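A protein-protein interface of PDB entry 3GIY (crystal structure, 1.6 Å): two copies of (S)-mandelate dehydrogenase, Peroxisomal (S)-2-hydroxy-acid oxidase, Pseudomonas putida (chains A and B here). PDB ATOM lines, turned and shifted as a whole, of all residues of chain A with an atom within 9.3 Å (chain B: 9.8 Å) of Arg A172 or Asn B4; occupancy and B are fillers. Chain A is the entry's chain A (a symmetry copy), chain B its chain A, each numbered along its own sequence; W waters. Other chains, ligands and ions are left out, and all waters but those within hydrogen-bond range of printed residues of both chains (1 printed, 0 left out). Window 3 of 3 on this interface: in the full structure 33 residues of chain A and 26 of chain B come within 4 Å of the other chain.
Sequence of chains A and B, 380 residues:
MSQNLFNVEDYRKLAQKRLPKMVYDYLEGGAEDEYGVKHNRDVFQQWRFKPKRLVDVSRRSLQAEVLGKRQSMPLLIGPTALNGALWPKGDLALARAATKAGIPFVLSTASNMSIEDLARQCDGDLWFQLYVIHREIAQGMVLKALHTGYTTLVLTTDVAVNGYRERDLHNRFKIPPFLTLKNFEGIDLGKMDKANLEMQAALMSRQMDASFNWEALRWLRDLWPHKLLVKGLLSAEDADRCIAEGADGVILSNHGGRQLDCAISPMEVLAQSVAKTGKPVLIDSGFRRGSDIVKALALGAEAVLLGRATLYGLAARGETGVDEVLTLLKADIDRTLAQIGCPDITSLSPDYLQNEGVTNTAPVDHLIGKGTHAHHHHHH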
ATOM      1  N   MET A  22     -24.374  28.376 -39.869  1.00  0.00           N
ATOM      2  CA  MET A  22     -23.619  29.322 -39.057  1.00  0.00           C
ATOM      3  C   MET A  22     -24.121  30.753 -39.253  1.00  0.00           C
ATOM      4  O   MET A  22     -24.210  31.527 -38.296  1.00  0.00           O
ATOM      5  CB  MET A  22     -22.133  29.230 -39.409  1.00  0.00           C
ATOM      6  CG  MET A  22     -21.216  30.038 -38.507  1.00  0.00           C
ATOM      7  SD  MET A  22     -19.504  29.971 -39.088  1.00  0.00           S
ATOM      8  CE  MET A  22     -19.034  28.330 -38.557  1.00  0.00           C
ATOM      9  N   ASP A  25     -27.704  31.069 -37.830  1.00  0.00           N
ATOM     10  CA  ASP A  25     -27.643  31.188 -36.373  1.00  0.00           C
ATOM     11  C   ASP A  25     -27.147  32.561 -35.930  1.00  0.00           C
ATOM     12  O   ASP A  25     -27.542  33.060 -34.877  1.00  0.00           O
ATOM     13  CB  ASP A  25     -26.761  30.085 -35.772  1.00  0.00           C
ATOM     14  CG  ASP A  25     -27.440  28.719 -35.790  1.00  0.00           C
ATOM     15  OD1 ASP A  25     -28.689  28.670 -35.814  1.00  0.00           O
ATOM     16  OD2 ASP A  25     -26.730  27.695 -35.762  1.00  0.00           O
ATOM     17  N   TYR A  26     -26.273  33.172 -36.729  1.00  0.00           N
ATOM     18  CA  TYR A  26     -25.777  34.510 -36.411  1.00  0.00           C
ATOM     19  C   TYR A  26     -26.943  35.502 -36.481  1.00  0.00           C
ATOM     20  O   TYR A  26     -27.043  36.419 -35.670  1.00  0.00           O
ATOM     21  CB  TYR A  26     -24.694  34.937 -37.409  1.00  0.00           C
ATOM     22  CG  TYR A  26     -24.488  36.437 -37.469  1.00  0.00           C
ATOM     23  CD1 TYR A  26     -23.976  37.138 -36.377  1.00  0.00           C
ATOM     24  CD2 TYR A  26     -24.843  37.163 -38.606  1.00  0.00           C
ATOM     25  CE1 TYR A  26     -23.828  38.528 -36.418  1.00  0.00           C
ATOM     26  CE2 TYR A  26     -24.695  38.551 -38.657  1.00  0.00           C
ATOM     27  CZ  TYR A  26     -24.190  39.223 -37.562  1.00  0.00           C
ATOM     28  OH  TYR A  26     -24.055  40.588 -37.613  1.00  0.00           O
ATOM     29  N   TYR A 164     -23.839  37.444 -24.853  1.00  0.00           N
ATOM     30  CA  TYR A 164     -23.429  36.046 -24.790  1.00  0.00           C
ATOM     31  C   TYR A 164     -24.371  35.189 -25.636  1.00  0.00           C
ATOM     32  O   TYR A 164     -25.329  34.613 -25.122  1.00  0.00           O
ATOM     33  CB  TYR A 164     -23.445  35.556 -23.339  1.00  0.00           C
ATOM     34  CG  TYR A 164     -22.585  34.337 -23.075  1.00  0.00           C
ATOM     35  CD1 TYR A 164     -21.189  34.411 -23.160  1.00  0.00           C
ATOM     36  CD2 TYR A 164     -23.157  33.119 -22.707  1.00  0.00           C
ATOM     37  CE1 TYR A 164     -20.386  33.303 -22.878  1.00  0.00           C
ATOM     38  CE2 TYR A 164     -22.363  31.999 -22.424  1.00  0.00           C
ATOM     39  CZ  TYR A 164     -20.980  32.100 -22.506  1.00  0.00           C
ATOM     40  OH  TYR A 164     -20.188  31.013 -22.196  1.00  0.00           O
ATOM     41  N   ARG A 165     -24.094  35.121 -26.936  1.00  0.00           N
ATOM     42  CA  ARG A 165     -24.909  34.336 -27.852  1.00  0.00           C
ATOM     43  C   ARG A 165     -24.241  32.986 -28.078  1.00  0.00           C
ATOM     44  O   ARG A 165     -23.279  32.859 -28.842  1.00  0.00           O
ATOM     45  CB  ARG A 165     -25.099  35.100 -29.164  1.00  0.00           C
ATOM     46  CG  ARG A 165     -25.850  36.416 -28.964  1.00  0.00           C
ATOM     47  CD  ARG A 165     -26.402  36.957 -30.266  1.00  0.00           C
ATOM     48  NE  ARG A 165     -25.402  37.667 -31.060  1.00  0.00           N
ATOM     49  CZ  ARG A 165     -24.991  38.908 -30.818  1.00  0.00           C
ATOM     50  NH1 ARG A 165     -25.486  39.600 -29.798  1.00  0.00           N
ATOM     51  NH2 ARG A 165     -24.087  39.464 -31.610  1.00  0.00           N
ATOM     52  N   GLU A 166     -24.777  31.981 -27.392  1.00  0.00           N
ATOM     53  CA  GLU A 166     -24.248  30.626 -27.415  1.00  0.00           C
ATOM     54  C   GLU A 166     -24.290  29.891 -28.759  1.00  0.00           C
ATOM     55  O   GLU A 166     -23.496  28.975 -28.981  1.00  0.00           O
ATOM     56  CB  GLU A 166     -24.918  29.831 -26.288  1.00  0.00           C
ATOM     57  CG  GLU A 166     -24.761  30.574 -24.960  1.00  0.00           C
ATOM     58  CD  GLU A 166     -25.477  29.942 -23.778  1.00  0.00           C
ATOM     59  OE1 GLU A 166     -26.523  29.291 -23.971  1.00  0.00           O
ATOM     60  OE2 GLU A 166     -24.998  30.127 -22.641  1.00  0.00           O
ATOM     61  N   ARG A 167     -25.185  30.285 -29.663  1.00  0.00           N
ATOM     62  CA  ARG A 167     -25.211  29.643 -30.976  1.00  0.00           C
ATOM     63  C   ARG A 167     -23.862  29.902 -31.655  1.00  0.00           C
ATOM     64  O   ARG A 167     -23.271  28.997 -32.234  1.00  0.00           O
ATOM     65  CB  ARG A 167     -26.327  30.204 -31.859  1.00  0.00           C
ATOM     66  CG  ARG A 167     -27.732  29.876 -31.406  1.00  0.00           C
ATOM     67  CD  ARG A 167     -28.723  30.138 -32.532  1.00  0.00           C
ATOM     68  NE  ARG A 167     -30.102  30.096 -32.069  1.00  0.00           N
ATOM     69  CZ  ARG A 167     -31.148  29.852 -32.853  1.00  0.00           C
ATOM     70  NH1 ARG A 167     -30.980  29.624 -34.151  1.00  0.00           N
ATOM     71  NH2 ARG A 167     -32.368  29.833 -32.335  1.00  0.00           N
ATOM     72  N   ASP A 168     -23.383  31.144 -31.577  1.00  0.00           N
ATOM     73  CA  ASP A 168     -22.098  31.525 -32.174  1.00  0.00           C
ATOM     74  C   ASP A 168     -20.954  30.757 -31.527  1.00  0.00           C
ATOM     75  O   ASP A 168     -20.019  30.336 -32.208  1.00  0.00           O
ATOM     76  CB  ASP A 168     -21.836  33.032 -32.017  1.00  0.00           C
ATOM     77  CG  ASP A 168     -22.817  33.889 -32.806  1.00  0.00           C
ATOM     78  OD1 ASP A 168     -23.329  33.417 -33.844  1.00  0.00           O
ATOM     79  OD2 ASP A 168     -23.057  35.046 -32.400  1.00  0.00           O
ATOM     80  N   LEU A 169     -21.030  30.591 -30.209  1.00  0.00           N
ATOM     81  CA  LEU A 169     -20.009  29.862 -29.462  1.00  0.00           C
ATOM     82  C   LEU A 169     -19.941  28.415 -29.933  1.00  0.00           C
ATOM     83  O   LEU A 169     -18.857  27.861 -30.114  1.00  0.00           O
ATOM     84  CB  LEU A 169     -20.320  29.901 -27.965  1.00  0.00           C
ATOM     85  CG  LEU A 169     -20.366  31.300 -27.350  1.00  0.00           C
ATOM     86  CD1 LEU A 169     -20.648  31.220 -25.859  1.00  0.00           C
ATOM     87  CD2 LEU A 169     -19.043  31.989 -27.608  1.00  0.00           C
ATOM     88  N   HIS A 170     -21.105  27.806 -30.134  1.00  0.00           N
ATOM     89  CA  HIS A 170     -21.171  26.427 -30.599  1.00  0.00           C
ATOM     90  C   HIS A 170     -20.672  26.287 -32.036  1.00  0.00           C
ATOM     91  O   HIS A 170     -20.107  25.257 -32.394  1.00  0.00           O
ATOM     92  CB  HIS A 170     -22.605  25.906 -30.497  1.00  0.00           C
ATOM     93  CG  HIS A 170     -23.059  25.668 -29.090  1.00  0.00           C
ATOM     94  ND1 HIS A 170     -24.329  25.981 -28.654  1.00  0.00           N
ATOM     95  CD2 HIS A 170     -22.418  25.132 -28.024  1.00  0.00           C
ATOM     96  CE1 HIS A 170     -24.449  25.651 -27.380  1.00  0.00           C
ATOM     97  NE2 HIS A 170     -23.304  25.132 -26.974  1.00  0.00           N
ATOM     98  N   ASN A 171     -20.888  27.313 -32.857  1.00  0.00           N
ATOM     99  CA  ASN A 171     -20.441  27.286 -34.251  1.00  0.00           C
ATOM    100  C   ASN A 171     -19.085  27.957 -34.415  1.00  0.00           C
ATOM    101  O   ASN A 171     -18.560  28.019 -35.527  1.00  0.00           O
ATOM    102  CB  ASN A 171     -21.420  28.021 -35.179  1.00  0.00           C
ATOM    103  CG  ASN A 171     -22.814  27.446 -35.148  1.00  0.00           C
ATOM    104  OD1 ASN A 171     -23.003  26.238 -34.998  1.00  0.00           O
ATOM    105  ND2 ASN A 171     -23.808  28.314 -35.315  1.00  0.00           N
ATOM    106  N   ARG A 172     -18.518  28.458 -33.318  1.00  0.00           N
ATOM    107  CA  ARG A 172     -17.239  29.163 -33.378  1.00  0.00           C
ATOM    108  C   ARG A 172     -17.369  30.190 -34.496  1.00  0.00           C
ATOM    109  O   ARG A 172     -16.458  30.372 -35.312  1.00  0.00           O
ATOM    110  CB  ARG A 172     -16.088  28.199 -33.679  1.00  0.00           C
ATOM    111  CG  ARG A 172     -15.566  27.439 -32.468  1.00  0.00           C
ATOM    112  CD  ARG A 172     -16.624  26.531 -31.860  1.00  0.00           C
ATOM    113  NE  ARG A 172     -16.127  25.835 -30.675  1.00  0.00           N
ATOM    114  CZ  ARG A 172     -16.844  24.986 -29.949  1.00  0.00           C
ATOM    115  NH1 ARG A 172     -18.100  24.723 -30.284  1.00  0.00           N
ATOM    116  NH2 ARG A 172     -16.309  24.402 -28.883  1.00  0.00           N
ATOM    117  N   PHE A 173     -18.524  30.852 -34.522  1.00  0.00           N
ATOM    118  CA  PHE A 173     -18.819  31.847 -35.535  1.00  0.00           C
ATOM    119  C   PHE A 173     -17.719  32.874 -35.720  1.00  0.00           C
ATOM    120  O   PHE A 173     -17.321  33.564 -34.777  1.00  0.00           O
ATOM    121  CB  PHE A 173     -20.122  32.583 -35.223  1.00  0.00           C
ATOM    122  CG  PHE A 173     -20.443  33.669 -36.213  1.00  0.00           C
ATOM    123  CD1 PHE A 173     -20.785  33.351 -37.523  1.00  0.00           C
ATOM    124  CD2 PHE A 173     -20.342  35.009 -35.854  1.00  0.00           C
ATOM    125  CE1 PHE A 173     -21.020  34.353 -38.463  1.00  0.00           C
ATOM    126  CE2 PHE A 173     -20.574  36.018 -36.785  1.00  0.00           C
ATOM    127  CZ  PHE A 173     -20.912  35.689 -38.092  1.00  0.00           C
ATOM    128  N   LYS A 174     -17.247  32.964 -36.958  1.00  0.00           N
ATOM    129  CA  LYS A 174     -16.207  33.904 -37.346  1.00  0.00           C
ATOM    130  C   LYS A 174     -16.749  34.725 -38.517  1.00  0.00           C
ATOM    131  O   LYS A 174     -17.270  34.166 -39.491  1.00  0.00           O
ATOM    132  CB  LYS A 174     -14.941  33.151 -37.773  1.00  0.00           C
ATOM    133  N   ILE A 175     -16.640  36.046 -38.408  1.00  0.00           N
ATOM    134  CA  ILE A 175     -17.107  36.957 -39.454  1.00  0.00           C
ATOM    135  C   ILE A 175     -16.606  36.471 -40.823  1.00  0.00           C
ATOM    136  O   ILE A 175     -15.396  36.355 -41.040  1.00  0.00           O
ATOM    137  CB  ILE A 175     -16.578  38.395 -39.197  1.00  0.00           C
ATOM    138  CG1 ILE A 175     -16.903  38.822 -37.760  1.00  0.00           C
ATOM    139  CG2 ILE A 175     -17.203  39.371 -40.188  1.00  0.00           C
ATOM    140  CD1 ILE A 175     -16.248  40.120 -37.339  1.00  0.00           C
ATOM    141  N   PRO A 176     -17.531  36.184 -41.763  1.00  0.00           N
ATOM    142  CA  PRO A 176     -17.195  35.706 -43.112  1.00  0.00           C
ATOM    143  C   PRO A 176     -15.904  36.284 -43.709  1.00  0.00           C
ATOM    144  O   PRO A 176     -15.606  37.470 -43.550  1.00  0.00           O
ATOM    145  CB  PRO A 176     -18.438  36.072 -43.916  1.00  0.00           C
ATOM    146  CG  PRO A 176     -19.532  35.806 -42.924  1.00  0.00           C
ATOM    147  CD  PRO A 176     -18.982  36.435 -41.649  1.00  0.00           C
ATOM    148  N   ASN B   4     -18.377  21.560 -25.933  1.00  0.00           N
ATOM    149  CA  ASN B   4     -19.266  22.754 -25.774  1.00  0.00           C
ATOM    150  C   ASN B   4     -19.704  22.973 -24.334  1.00  0.00           C
ATOM    151  O   ASN B   4     -20.815  22.610 -23.949  1.00  0.00           O
ATOM    152  CB  ASN B   4     -20.512  22.617 -26.653  1.00  0.00           C
ATOM    153  CG  ASN B   4     -20.206  22.782 -28.126  1.00  0.00           C
ATOM    154  OD1 ASN B   4     -19.617  23.783 -28.541  1.00  0.00           O
ATOM    155  ND2 ASN B   4     -20.612  21.803 -28.930  1.00  0.00           N
ATOM    156  N   LEU B   5     -18.828  23.571 -23.540  1.00  0.00           N
ATOM    157  CA  LEU B   5     -19.140  23.844 -22.149  1.00  0.00           C
ATOM    158  C   LEU B   5     -19.127  25.359 -21.948  1.00  0.00           C
ATOM    159  O   LEU B   5     -18.129  25.950 -21.527  1.00  0.00           O
ATOM    160  CB  LEU B   5     -18.125  23.134 -21.254  1.00  0.00           C
ATOM    161  CG  LEU B   5     -18.207  21.603 -21.394  1.00  0.00           C
ATOM    162  CD1 LEU B   5     -17.044  20.934 -20.676  1.00  0.00           C
ATOM    163  CD2 LEU B   5     -19.527  21.115 -20.832  1.00  0.00           C
ATOM    164  N   PHE B   6     -20.264  25.980 -22.257  1.00  0.00           N
ATOM    165  CA  PHE B   6     -20.407  27.427 -22.167  1.00  0.00           C
ATOM    166  C   PHE B   6     -21.336  27.916 -21.059  1.00  0.00           C
ATOM    167  O   PHE B   6     -21.502  29.120 -20.872  1.00  0.00           O
ATOM    168  CB  PHE B   6     -20.878  27.964 -23.519  1.00  0.00           C
ATOM    169  CG  PHE B   6     -19.995  27.556 -24.667  1.00  0.00           C
ATOM    170  CD1 PHE B   6     -18.697  28.041 -24.772  1.00  0.00           C
ATOM    171  CD2 PHE B   6     -20.457  26.675 -25.637  1.00  0.00           C
ATOM    172  CE1 PHE B   6     -17.872  27.654 -25.828  1.00  0.00           C
ATOM    173  CE2 PHE B   6     -19.640  26.284 -26.695  1.00  0.00           C
ATOM    174  CZ  PHE B   6     -18.346  26.774 -26.790  1.00  0.00           C
ATOM    175  N   ASN B   7     -21.949  26.986 -20.334  1.00  0.00           N
ATOM    176  CA  ASN B   7     -22.839  27.350 -19.231  1.00  0.00           C
ATOM    177  C   ASN B   7     -23.068  26.164 -18.295  1.00  0.00           C
ATOM    178  O   ASN B   7     -22.602  25.053 -18.563  1.00  0.00           O
ATOM    179  CB  ASN B   7     -24.183  27.887 -19.755  1.00  0.00           C
ATOM    180  CG  ASN B   7     -24.965  26.862 -20.546  1.00  0.00           C
ATOM    181  OD1 ASN B   7     -25.087  25.708 -20.146  1.00  0.00           O
ATOM    182  ND2 ASN B   7     -25.524  27.290 -21.671  1.00  0.00           N
ATOM    183  N   VAL B   8     -23.783  26.402 -17.198  1.00  0.00           N
ATOM    184  CA  VAL B   8     -24.045  25.349 -16.221  1.00  0.00           C
ATOM    185  C   VAL B   8     -24.818  24.160 -16.800  1.00  0.00           C
ATOM    186  O   VAL B   8     -24.533  23.013 -16.450  1.00  0.00           O
ATOM    187  CB  VAL B   8     -24.788  25.919 -14.974  1.00  0.00           C
ATOM    188  CG1 VAL B   8     -25.131  24.797 -13.987  1.00  0.00           C
ATOM    189  CG2 VAL B   8     -23.906  26.949 -14.285  1.00  0.00           C
ATOM    190  N   GLU B   9     -25.779  24.426 -17.683  1.00  0.00           N
ATOM    191  CA  GLU B   9     -26.555  23.350 -18.297  1.00  0.00           C
ATOM    192  C   GLU B   9     -25.655  22.398 -19.082  1.00  0.00           C
ATOM    193  O   GLU B   9     -25.882  21.191 -19.094  1.00  0.00           O
ATOM    194  CB  GLU B   9     -27.629  23.921 -19.224  1.00  0.00           C
ATOM    195  CG  GLU B   9     -28.355  22.873 -20.054  1.00  0.00           C
ATOM    196  CD  GLU B   9     -29.244  21.951 -19.239  1.00  0.00           C
ATOM    197  OE1 GLU B   9     -29.169  21.959 -17.993  1.00  0.00           O
ATOM    198  OE2 GLU B   9     -30.025  21.202 -19.857  1.00  0.00           O
ATOM    199  N   ASP B  10     -24.640  22.948 -19.741  1.00  0.00           N
ATOM    200  CA  ASP B  10     -23.702  22.139 -20.507  1.00  0.00           C
ATOM    201  C   ASP B  10     -22.962  21.167 -19.594  1.00  0.00           C
ATOM    202  O   ASP B  10     -22.653  20.037 -19.988  1.00  0.00           O
ATOM    203  CB  ASP B  10     -22.704  23.030 -21.242  1.00  0.00           C
ATOM    204  CG  ASP B  10     -23.349  23.810 -22.375  1.00  0.00           C
ATOM    205  OD1 ASP B  10     -24.349  23.312 -22.933  1.00  0.00           O
ATOM    206  OD2 ASP B  10     -22.853  24.907 -22.719  1.00  0.00           O
ATOM    207  N   TYR B  11     -22.671  21.607 -18.373  1.00  0.00           N
ATOM    208  CA  TYR B  11     -21.997  20.737 -17.422  1.00  0.00           C
ATOM    209  C   TYR B  11     -22.957  19.681 -16.876  1.00  0.00           C
ATOM    210  O   TYR B  11     -22.542  18.551 -16.629  1.00  0.00           O
ATOM    211  CB  TYR B  11     -21.355  21.545 -16.283  1.00  0.00           C
ATOM    212  CG  TYR B  11     -20.038  22.166 -16.703  1.00  0.00           C
ATOM    213  CD1 TYR B  11     -20.006  23.377 -17.404  1.00  0.00           C
ATOM    214  CD2 TYR B  11     -18.827  21.498 -16.481  1.00  0.00           C
ATOM    215  CE1 TYR B  11     -18.808  23.901 -17.881  1.00  0.00           C
ATOM    216  CE2 TYR B  11     -17.622  22.014 -16.953  1.00  0.00           C
ATOM    217  CZ  TYR B  11     -17.622  23.213 -17.654  1.00  0.00           C
ATOM    218  OH  TYR B  11     -16.440  23.720 -18.149  1.00  0.00           O
ATOM    219  N   ARG B  12     -24.236  20.030 -16.698  1.00  0.00           N
ATOM    220  CA  ARG B  12     -25.206  19.042 -16.216  1.00  0.00           C
ATOM    221  C   ARG B  12     -25.259  17.903 -17.241  1.00  0.00           C
ATOM    222  O   ARG B  12     -25.195  16.730 -16.887  1.00  0.00           O
ATOM    223  CB  ARG B  12     -26.614  19.639 -16.073  1.00  0.00           C
ATOM    224  CG  ARG B  12     -27.629  18.644 -15.490  1.00  0.00           C
ATOM    225  CD  ARG B  12     -29.081  19.079 -15.695  1.00  0.00           C
ATOM    226  NE  ARG B  12     -29.416  19.229 -17.109  1.00  0.00           N
ATOM    227  CZ  ARG B  12     -29.461  18.227 -17.981  1.00  0.00           C
ATOM    228  NH1 ARG B  12     -29.196  16.990 -17.588  1.00  0.00           N
ATOM    229  NH2 ARG B  12     -29.762  18.464 -19.251  1.00  0.00           N
ATOM    230  N   LYS B  13     -25.373  18.270 -18.514  1.00  0.00           N
ATOM    231  CA  LYS B  13     -25.428  17.294 -19.596  1.00  0.00           C
ATOM    232  C   LYS B  13     -24.222  16.349 -19.581  1.00  0.00           C
ATOM    233  O   LYS B  13     -24.373  15.139 -19.759  1.00  0.00           O
ATOM    234  CB  LYS B  13     -25.520  18.021 -20.940  1.00  0.00           C
ATOM    235  CG  LYS B  13     -26.808  18.813 -21.090  1.00  0.00           C
ATOM    236  CD  LYS B  13     -26.844  19.646 -22.362  1.00  0.00           C
ATOM    237  CE  LYS B  13     -28.190  20.343 -22.500  1.00  0.00           C
ATOM    238  NZ  LYS B  13     -28.234  21.272 -23.655  1.00  0.00           N
ATOM    239  N   LEU B  14     -23.030  16.902 -19.364  1.00  0.00           N
ATOM    240  CA  LEU B  14     -21.812  16.094 -19.325  1.00  0.00           C
ATOM    241  C   LEU B  14     -21.806  15.206 -18.074  1.00  0.00           C
ATOM    242  O   LEU B  14     -21.393  14.043 -18.127  1.00  0.00           O
ATOM    243  CB  LEU B  14     -20.578  17.001 -19.333  1.00  0.00           C
ATOM    244  CG  LEU B  14     -19.221  16.313 -19.505  1.00  0.00           C
ATOM    245  CD1 LEU B  14     -19.209  15.540 -20.818  1.00  0.00           C
ATOM    246  CD2 LEU B  14     -18.103  17.351 -19.488  1.00  0.00           C
ATOM    247  N   LYS B  17     -23.839  12.163 -18.505  1.00  0.00           N
ATOM    248  CA  LYS B  17     -23.221  11.168 -19.372  1.00  0.00           C
ATOM    249  C   LYS B  17     -22.130  10.397 -18.641  1.00  0.00           C
ATOM    250  O   LYS B  17     -21.867   9.240 -18.958  1.00  0.00           O
ATOM    251  CB  LYS B  17     -22.622  11.833 -20.615  1.00  0.00           C
ATOM    252  CG  LYS B  17     -23.657  12.412 -21.563  1.00  0.00           C
ATOM    253  CD  LYS B  17     -23.031  12.906 -22.859  1.00  0.00           C
ATOM    254  CE  LYS B  17     -22.021  14.021 -22.613  1.00  0.00           C
ATOM    255  NZ  LYS B  17     -21.423  14.541 -23.882  1.00  0.00           N
ATOM    256  N   ARG B  18     -21.514  11.029 -17.646  1.00  0.00           N
ATOM    257  CA  ARG B  18     -20.428  10.394 -16.911  1.00  0.00           C
ATOM    258  C   ARG B  18     -20.791   9.682 -15.609  1.00  0.00           C
ATOM    259  O   ARG B  18     -20.098   8.750 -15.196  1.00  0.00           O
ATOM    260  CB  ARG B  18     -19.314  11.426 -16.680  1.00  0.00           C
ATOM    261  CG  ARG B  18     -18.788  11.981 -18.003  1.00  0.00           C
ATOM    262  CD  ARG B  18     -17.516  12.807 -17.888  1.00  0.00           C
ATOM    263  NE  ARG B  18     -16.996  13.126 -19.220  1.00  0.00           N
ATOM    264  CZ  ARG B  18     -15.935  13.891 -19.464  1.00  0.00           C
ATOM    265  NH1 ARG B  18     -15.260  14.435 -18.461  1.00  0.00           N
ATOM    266  NH2 ARG B  18     -15.544  14.108 -20.715  1.00  0.00           N
ATOM    267  N   ARG B 317     -16.003  17.055 -14.514  1.00  0.00           N
ATOM    268  CA  ARG B 317     -14.564  17.192 -14.699  1.00  0.00           C
ATOM    269  C   ARG B 317     -13.729  17.457 -13.447  1.00  0.00           C
ATOM    270  O   ARG B 317     -12.660  18.055 -13.534  1.00  0.00           O
ATOM    271  CB  ARG B 317     -14.299  18.289 -15.735  1.00  0.00           C
ATOM    272  CG  ARG B 317     -14.686  17.883 -17.151  1.00  0.00           C
ATOM    273  CD  ARG B 317     -14.769  19.074 -18.095  1.00  0.00           C
ATOM    274  NE  ARG B 317     -13.576  19.918 -18.062  1.00  0.00           N
ATOM    275  CZ  ARG B 317     -12.369  19.546 -18.481  1.00  0.00           C
ATOM    276  NH1 ARG B 317     -12.174  18.329 -18.976  1.00  0.00           N
ATOM    277  NH2 ARG B 317     -11.351  20.395 -18.403  1.00  0.00           N
ATOM    278  N   GLU B 324     -13.981  25.772 -13.776  1.00  0.00           N
ATOM    279  CA  GLU B 324     -14.603  26.231 -15.015  1.00  0.00           C
ATOM    280  C   GLU B 324     -16.004  26.788 -14.825  1.00  0.00           C
ATOM    281  O   GLU B 324     -16.367  27.784 -15.455  1.00  0.00           O
ATOM    282  CB  GLU B 324     -14.614  25.095 -16.034  1.00  0.00           C
ATOM    283  CG  GLU B 324     -13.213  24.543 -16.303  1.00  0.00           C
ATOM    284  CD  GLU B 324     -13.202  23.367 -17.261  1.00  0.00           C
ATOM    285  OE1 GLU B 324     -14.209  22.633 -17.307  1.00  0.00           O
ATOM    286  OE2 GLU B 324     -12.181  23.166 -17.955  1.00  0.00           O
ATOM    287  N   LEU B 328     -17.096  30.643 -15.457  1.00  0.00           N
ATOM    288  CA  LEU B 328     -18.217  31.008 -16.317  1.00  0.00           C
ATOM    289  C   LEU B 328     -19.219  31.871 -15.565  1.00  0.00           C
ATOM    290  O   LEU B 328     -19.679  32.888 -16.083  1.00  0.00           O
ATOM    291  CB  LEU B 328     -18.930  29.758 -16.843  1.00  0.00           C
ATOM    292  CG  LEU B 328     -18.189  28.953 -17.911  1.00  0.00           C
ATOM    293  CD1 LEU B 328     -18.952  27.667 -18.202  1.00  0.00           C
ATOM    294  CD2 LEU B 328     -18.037  29.797 -19.168  1.00  0.00           C
HETATM  295  O   HOH W   1     -24.265  26.300 -24.551  1.00  0.00           O
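ND2 of Asn B7 is in hydrogen-bond range of OE2 of Glu A166 (3.0 Å).
The side-chain amide oxygen (OD1) of Asn B4 sits at hydrogen-bond distance from the guanidinium group (NH1) of Arg A172 (2.5 Å).
The backbone carbonyl oxygen (O) of Phe B6 sits at hydrogen-bond distance from the side-chain hydroxyl (OH) of Tyr A164 (2.7 Å).
The backbone carbonyl oxygen (O) of Leu A169 sits close to the guanidinium group (NH1) of Arg A172 (3.2 Å).
The backbone NH (N) of Phe B6 lies within hydrogen-bond range of the side-chain carboxylate (OD2) of Asp B10, at 2.8 Å.
OD1 of Asn B7 lies within hydrogen-bond range of N of Glu B9, 2.9 Å away.
The backbone carbonyl oxygen of Glu A166 lies within hydrogen-bond range of a ring nitrogen (ND1) of His A170 (3.1 Å).
The side-chain amide oxygen of Asn B7 lies within hydrogen-bond range of the backbone NH of Asp B10, at 2.8 Å.
The backbone carbonyl oxygen (O) of His A170 sits at hydrogen-bond distance from the guanidinium group (NH1) of Arg A172 (3.0 Å).
Among the printed residues, pairs that only touch across the chains: His A170 with Asn B4 (3.2 Å), His A170 with Phe B6 (3.3 Å), Leu A169 with Phe B6 (3.5 Å), Arg A172 with Phe B6 (3.8 Å) and Tyr A164 with Leu B328 (3.9 Å).
Of the printed residues of chain B, Glu A166 touches Asn B7.
Of chain B, only Asn B4 and Phe B6 come within 4 Å of His A170.
No residue of chain B comes within 4 Å of Asn A171.
Of chain B, only Asn B4 and Phe B6 come within 4 Å of Arg A172.
No residue of chain B comes within 4 Å of Lys A174.
No residue of chain A comes within 4 Å of Leu B5.
Of the printed residues of chain A, Phe B6 touches Tyr A164, Leu A169, His A170 and Arg A172.
Printed residues of chain A within 4 Å of Asn B7: Glu A166 (3.0 Å).
Tyr B11 touches none of the printed residues of chain A.
Arg B12 touches none of the printed residues of chain A.
The nearest residue of chain B that does not touch Arg A172 is Leu B5 (6.0 Å).
Of the 16 printed residues of chain B, 4 touch a printed residue of chain A.
Hydrophobic or aromatic side chains of chain B that line the printed part of chain A: Phe B6 and Leu B328.
Along chain A the printed residues that touch a printed residue of chain B span positions 164 to 172.
Among the printed residues, no Asp or Glu carboxylate lies within 4 Å of a Lys or Arg side-chain nitrogen of the other chain.
No position is printed for both chains.
Water W1 lies within hydrogen-bond range of the side-chain carboxylate (OD2) of Asp B10, a ring nitrogen (NE2) of His A170 and the side-chain amide nitrogen (ND2) of Asn B7.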
